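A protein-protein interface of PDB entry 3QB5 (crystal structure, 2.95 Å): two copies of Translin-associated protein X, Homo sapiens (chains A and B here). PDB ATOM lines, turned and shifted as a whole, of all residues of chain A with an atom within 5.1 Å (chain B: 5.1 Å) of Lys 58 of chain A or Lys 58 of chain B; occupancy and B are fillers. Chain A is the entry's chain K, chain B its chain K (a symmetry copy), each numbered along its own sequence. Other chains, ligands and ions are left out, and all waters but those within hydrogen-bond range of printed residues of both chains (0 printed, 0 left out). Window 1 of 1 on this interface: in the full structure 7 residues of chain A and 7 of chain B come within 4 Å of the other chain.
The guanidinium group (NH2) of Arg 61 of chain B is in salt-bridge range of the side-chain carboxylate (OE1) of Glu 54 of chain A (3.0 Å).
NZ of Lys 58 of chain A lies within salt-bridge range of OD2 of Asp 62 of chain B (3.3 Å).
The side-chain carboxylate (OE1) of Glu 54 of chain B is in salt-bridge range of the guanidinium group (NH2) of Arg 61 of chain A, 3.0 Å away.
OD2 of Asp 62 of chain A is in salt-bridge range of NZ of Lys 58 of chain B (3.3 Å).
Glu 54 of chain A touches Arg 61 of chain B, and with the chains exchanged Arg 61 of chain A touches Glu 54 of chain B.
Lys 58 of chain A touches its own counterpart, Lys 58 of chain B.
Lys 58 of chain A touches Asp 62 of chain B, and with the chains exchanged Asp 62 of chain A touches Lys 58 of chain B.
Of the 9 printed residues of chain B, 4 touch a printed residue of chain A.
Among the printed residues, 5 pairs touch across the chains.
Among the printed residues, Asp or Glu carboxylates within 4 Å of a Lys or Arg side-chain nitrogen of the other chain: Glu 54 of chain A with Arg 61 of chain B, Lys 58 of chain A with Asp 62 of chain B, Arg 61 of chain A with Glu 54 of chain B and Asp 62 of chain A with Lys 58 of chain B.
Lys 58 of chain A touches Lys 58 of chain B (CD to CD, 3.8 Å).
Of chain B, only Lys 58 (3.8 Å) and Asp 62 (3.3 Å) come within 4 Å of Lys 58 of chain A.
Lys 58 of chain B touches just these residues of chain A: Lys 58 (3.8 Å) and Asp 62 (3.3 Å).
Of the printed residues of chain B, Asp 62 of chain A touches Lys 58 (3.3 Å).
Of the printed residues of chain A, Arg 61 of chain B touches Glu 54 (3.0 Å).
Of the printed residues of chain A, Glu 54 of chain B touches Arg 61 (3.0 Å).
Of the printed residues of chain A, Asp 62 of chain B touches Lys 58.
Of the printed residues of chain B, Arg 61 of chain A touches Glu 54.
The nearest printed residue of chain A that does not touch Lys 58 of chain B is Arg 61 of chain A (5.3 Å).
The nearest printed residue of chain A that does not touch Asp 62 of chain B is Glu 54 of chain A (5.7 Å).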
ATOM      1  N   GLU A  54       3.487 -34.219  31.829  1.00  0.00           N
ATOM      2  CA  GLU A  54       2.809 -33.170  31.071  1.00  0.00           C
ATOM      3  C   GLU A  54       3.760 -32.460  30.101  1.00  0.00           C
ATOM      4  O   GLU A  54       3.388 -32.133  28.963  1.00  0.00           O
ATOM      5  CB  GLU A  54       2.147 -32.162  32.016  1.00  0.00           C
ATOM      6  CG  GLU A  54       0.970 -32.730  32.802  1.00  0.00           C
ATOM      7  CD  GLU A  54      -0.192 -33.137  31.907  1.00  0.00           C
ATOM      8  OE1 GLU A  54      -0.735 -34.248  32.097  1.00  0.00           O
ATOM      9  OE2 GLU A  54      -0.565 -32.342  31.015  1.00  0.00           O
ATOM     10  N   ARG A  55       4.989 -32.231  30.552  1.00  0.00           N
ATOM     11  CA  ARG A  55       6.002 -31.605  29.712  1.00  0.00           C
ATOM     12  C   ARG A  55       6.322 -32.464  28.492  1.00  0.00           C
ATOM     13  O   ARG A  55       6.470 -31.950  27.381  1.00  0.00           O
ATOM     14  CB  ARG A  55       7.270 -31.338  30.522  1.00  0.00           C
ATOM     15  CG  ARG A  55       7.496 -29.870  30.862  1.00  0.00           C
ATOM     16  CD  ARG A  55       8.018 -29.709  32.283  1.00  0.00           C
ATOM     17  NE  ARG A  55       9.052 -30.690  32.600  1.00  0.00           N
ATOM     18  CZ  ARG A  55       9.382 -31.045  33.835  1.00  0.00           C
ATOM     19  NH1 ARG A  55       8.758 -30.498  34.870  1.00  0.00           N
ATOM     20  NH2 ARG A  55      10.331 -31.949  34.036  1.00  0.00           N
ATOM     21  N   LEU A  56       6.429 -33.772  28.704  1.00  0.00           N
ATOM     22  CA  LEU A  56       6.687 -34.712  27.615  1.00  0.00           C
ATOM     23  C   LEU A  56       5.493 -34.833  26.665  1.00  0.00           C
ATOM     24  O   LEU A  56       5.644 -35.212  25.503  1.00  0.00           O
ATOM     25  CB  LEU A  56       7.056 -36.088  28.172  1.00  0.00           C
ATOM     26  CG  LEU A  56       8.448 -36.219  28.783  1.00  0.00           C
ATOM     27  CD1 LEU A  56       8.548 -37.495  29.594  1.00  0.00           C
ATOM     28  CD2 LEU A  56       9.507 -36.181  27.700  1.00  0.00           C
ATOM     29  N   VAL A  57       4.309 -34.512  27.171  1.00  0.00           N
ATOM     30  CA  VAL A  57       3.094 -34.544  26.371  1.00  0.00           C
ATOM     31  C   VAL A  57       3.062 -33.350  25.425  1.00  0.00           C
ATOM     32  O   VAL A  57       2.675 -33.482  24.267  1.00  0.00           O
ATOM     33  CB  VAL A  57       1.835 -34.568  27.262  1.00  0.00           C
ATOM     34  CG1 VAL A  57       0.601 -34.213  26.463  1.00  0.00           C
ATOM     35  CG2 VAL A  57       1.681 -35.931  27.906  1.00  0.00           C
ATOM     36  N   LYS A  58       3.481 -32.188  25.920  1.00  0.00           N
ATOM     37  CA  LYS A  58       3.565 -30.996  25.080  1.00  0.00           C
ATOM     38  C   LYS A  58       4.670 -31.125  24.030  1.00  0.00           C
ATOM     39  O   LYS A  58       4.485 -30.756  22.866  1.00  0.00           O
ATOM     40  CB  LYS A  58       3.795 -29.749  25.933  1.00  0.00           C
ATOM     41  CG  LYS A  58       2.661 -29.430  26.886  1.00  0.00           C
ATOM     42  CD  LYS A  58       2.923 -28.133  27.633  1.00  0.00           C
ATOM     43  CE  LYS A  58       1.786 -27.803  28.584  1.00  0.00           C
ATOM     44  NZ  LYS A  58       2.012 -26.508  29.285  1.00  0.00           N
ATOM     45  N   LEU A  59       5.819 -31.646  24.448  1.00  0.00           N
ATOM     46  CA  LEU A  59       6.920 -31.885  23.524  1.00  0.00           C
ATOM     47  C   LEU A  59       6.511 -32.861  22.429  1.00  0.00           C
ATOM     48  O   LEU A  59       6.844 -32.670  21.261  1.00  0.00           O
ATOM     49  CB  LEU A  59       8.148 -32.420  24.265  1.00  0.00           C
ATOM     50  CG  LEU A  59       9.225 -31.405  24.656  1.00  0.00           C
ATOM     51  CD1 LEU A  59       8.671 -30.345  25.603  1.00  0.00           C
ATOM     52  CD2 LEU A  59      10.407 -32.119  25.277  1.00  0.00           C
ATOM     53  N   SER A  60       5.786 -33.907  22.816  1.00  0.00           N
ATOM     54  CA  SER A  60       5.328 -34.921  21.874  1.00  0.00           C
ATOM     55  C   SER A  60       4.274 -34.365  20.922  1.00  0.00           C
ATOM     56  O   SER A  60       4.173 -34.792  19.773  1.00  0.00           O
ATOM     57  CB  SER A  60       4.768 -36.129  22.621  1.00  0.00           C
ATOM     58  OG  SER A  60       4.405 -37.155  21.717  1.00  0.00           O
ATOM     59  N   ARG A  61       3.486 -33.413  21.409  1.00  0.00           N
ATOM     60  CA  ARG A  61       2.473 -32.775  20.587  1.00  0.00           C
ATOM     61  C   ARG A  61       3.141 -31.931  19.518  1.00  0.00           C
ATOM     62  O   ARG A  61       2.679 -31.879  18.382  1.00  0.00           O
ATOM     63  CB  ARG A  61       1.557 -31.896  21.434  1.00  0.00           C
ATOM     64  CG  ARG A  61       0.386 -31.318  20.657  1.00  0.00           C
ATOM     65  CD  ARG A  61      -0.525 -32.422  20.158  1.00  0.00           C
ATOM     66  NE  ARG A  61      -1.602 -31.920  19.311  1.00  0.00           N
ATOM     67  CZ  ARG A  61      -1.739 -32.213  18.020  1.00  0.00           C
ATOM     68  NH1 ARG A  61      -0.866 -33.011  17.420  1.00  0.00           N
ATOM     69  NH2 ARG A  61      -2.753 -31.710  17.330  1.00  0.00           N
ATOM     70  N   ASP A  62       4.231 -31.265  19.886  1.00  0.00           N
ATOM     71  CA  ASP A  62       4.960 -30.436  18.933  1.00  0.00           C
ATOM     72  C   ASP A  62       5.684 -31.289  17.898  1.00  0.00           C
ATOM     73  O   ASP A  62       5.720 -30.949  16.716  1.00  0.00           O
ATOM     74  CB  ASP A  62       5.943 -29.520  19.658  1.00  0.00           C
ATOM     75  CG  ASP A  62       5.259 -28.599  20.648  1.00  0.00           C
ATOM     76  OD1 ASP A  62       4.068 -28.278  20.442  1.00  0.00           O
ATOM     77  OD2 ASP A  62       5.911 -28.197  21.634  1.00  0.00           O
ATOM     78  N   GLU B  54      -3.542 -24.888  19.421  1.00  0.00           N
ATOM     79  CA  GLU B  54      -2.626 -25.684  20.235  1.00  0.00           C
ATOM     80  C   GLU B  54      -2.220 -24.954  21.519  1.00  0.00           C
ATOM     81  O   GLU B  54      -2.113 -25.562  22.596  1.00  0.00           O
ATOM     82  CB  GLU B  54      -1.389 -26.082  19.423  1.00  0.00           C
ATOM     83  CG  GLU B  54      -1.677 -27.069  18.297  1.00  0.00           C
ATOM     84  CD  GLU B  54      -2.166 -28.416  18.809  1.00  0.00           C
ATOM     85  OE1 GLU B  54      -3.163 -28.940  18.262  1.00  0.00           O
ATOM     86  OE2 GLU B  54      -1.552 -28.954  19.757  1.00  0.00           O
ATOM     87  N   ARG B  55      -2.003 -23.648  21.404  1.00  0.00           N
ATOM     88  CA  ARG B  55      -1.657 -22.830  22.559  1.00  0.00           C
ATOM     89  C   ARG B  55      -2.779 -22.822  23.593  1.00  0.00           C
ATOM     90  O   ARG B  55      -2.527 -22.912  24.796  1.00  0.00           O
ATOM     91  CB  ARG B  55      -1.330 -21.403  22.118  1.00  0.00           C
ATOM     92  CG  ARG B  55       0.153 -21.057  22.175  1.00  0.00           C
ATOM     93  CD  ARG B  55       0.568 -20.223  20.972  1.00  0.00           C
ATOM     94  NE  ARG B  55      -0.406 -19.178  20.668  1.00  0.00           N
ATOM     95  CZ  ARG B  55      -0.516 -18.589  19.484  1.00  0.00           C
ATOM     96  NH1 ARG B  55       0.289 -18.945  18.491  1.00  0.00           N
ATOM     97  NH2 ARG B  55      -1.432 -17.651  19.291  1.00  0.00           N
ATOM     98  N   LEU B  56      -4.016 -22.715  23.118  1.00  0.00           N
ATOM     99  CA  LEU B  56      -5.185 -22.741  23.997  1.00  0.00           C
ATOM    100  C   LEU B  56      -5.405 -24.122  24.619  1.00  0.00           C
ATOM    101  O   LEU B  56      -6.034 -24.250  25.670  1.00  0.00           O
ATOM    102  CB  LEU B  56      -6.436 -22.303  23.235  1.00  0.00           C
ATOM    103  CG  LEU B  56      -6.550 -20.814  22.920  1.00  0.00           C
ATOM    104  CD1 LEU B  56      -7.628 -20.576  21.882  1.00  0.00           C
ATOM    105  CD2 LEU B  56      -6.831 -20.027  24.184  1.00  0.00           C
ATOM    106  N   VAL B  57      -4.886 -25.150  23.958  1.00  0.00           N
ATOM    107  CA  VAL B  57      -4.986 -26.515  24.453  1.00  0.00           C
ATOM    108  C   VAL B  57      -4.023 -26.719  25.615  1.00  0.00           C
ATOM    109  O   VAL B  57      -4.365 -27.362  26.604  1.00  0.00           O
ATOM    110  CB  VAL B  57      -4.716 -27.540  23.333  1.00  0.00           C
ATOM    111  CG1 VAL B  57      -4.438 -28.910  23.910  1.00  0.00           C
ATOM    112  CG2 VAL B  57      -5.893 -27.590  22.381  1.00  0.00           C
ATOM    113  N   LYS B  58      -2.821 -26.160  25.496  1.00  0.00           N
ATOM    114  CA  LYS B  58      -1.846 -26.228  26.581  1.00  0.00           C
ATOM    115  C   LYS B  58      -2.287 -25.394  27.786  1.00  0.00           C
ATOM    116  O   LYS B  58      -2.160 -25.824  28.936  1.00  0.00           O
ATOM    117  CB  LYS B  58      -0.470 -25.769  26.101  1.00  0.00           C
ATOM    118  CG  LYS B  58       0.138 -26.647  25.026  1.00  0.00           C
ATOM    119  CD  LYS B  58       1.537 -26.180  24.665  1.00  0.00           C
ATOM    120  CE  LYS B  58       2.155 -27.061  23.593  1.00  0.00           C
ATOM    121  NZ  LYS B  58       3.546 -26.638  23.267  1.00  0.00           N
ATOM    122  N   LEU B  59      -2.801 -24.198  27.515  1.00  0.00           N
ATOM    123  CA  LEU B  59      -3.321 -23.343  28.574  1.00  0.00           C
ATOM    124  C   LEU B  59      -4.470 -24.022  29.308  1.00  0.00           C
ATOM    125  O   LEU B  59      -4.561 -23.955  30.531  1.00  0.00           O
ATOM    126  CB  LEU B  59      -3.787 -21.998  28.010  1.00  0.00           C
ATOM    127  CG  LEU B  59      -2.805 -20.827  28.096  1.00  0.00           C
ATOM    128  CD1 LEU B  59      -1.526 -21.116  27.317  1.00  0.00           C
ATOM    129  CD2 LEU B  59      -3.466 -19.560  27.595  1.00  0.00           C
ATOM    130  N   SER B  60      -5.347 -24.675  28.549  1.00  0.00           N
ATOM    131  CA  SER B  60      -6.496 -25.367  29.118  1.00  0.00           C
ATOM    132  C   SER B  60      -6.069 -26.590  29.925  1.00  0.00           C
ATOM    133  O   SER B  60      -6.721 -26.962  30.899  1.00  0.00           O
ATOM    134  CB  SER B  60      -7.466 -25.785  28.016  1.00  0.00           C
ATOM    135  OG  SER B  60      -8.628 -26.378  28.567  1.00  0.00           O
ATOM    136  N   ARG B  61      -4.974 -27.215  29.509  1.00  0.00           N
ATOM    137  CA  ARG B  61      -4.443 -28.365  30.220  1.00  0.00           C
ATOM    138  C   ARG B  61      -3.904 -27.928  31.568  1.00  0.00           C
ATOM    139  O   ARG B  61      -4.056 -28.633  32.561  1.00  0.00           O
ATOM    140  CB  ARG B  61      -3.331 -29.037  29.418  1.00  0.00           C
ATOM    141  CG  ARG B  61      -2.837 -30.332  30.038  1.00  0.00           C
ATOM    142  CD  ARG B  61      -3.941 -31.370  30.069  1.00  0.00           C
ATOM    143  NE  ARG B  61      -3.543 -32.592  30.759  1.00  0.00           N
ATOM    144  CZ  ARG B  61      -4.091 -33.027  31.891  1.00  0.00           C
ATOM    145  NH1 ARG B  61      -5.069 -32.339  32.467  1.00  0.00           N
ATOM    146  NH2 ARG B  61      -3.665 -34.153  32.445  1.00  0.00           N
ATOM    147  N   ASP B  62      -3.268 -26.762  31.600  1.00  0.00           N
ATOM    148  CA  ASP B  62      -2.725 -26.239  32.848  1.00  0.00           C
ATOM    149  C   ASP B  62      -3.835 -25.796  33.794  1.00  0.00           C
ATOM    150  O   ASP B  62      -3.758 -26.017  35.002  1.00  0.00           O
ATOM    151  CB  ASP B  62      -1.759 -25.087  32.575  1.00  0.00           C
ATOM    152  CG  ASP B  62      -0.595 -25.499  31.697  1.00  0.00           C
ATOM    153  OD1 ASP B  62      -0.228 -26.694  31.711  1.00  0.00           O
ATOM    154  OD2 ASP B  62      -0.049 -24.628  30.989  1.00  0.00           O
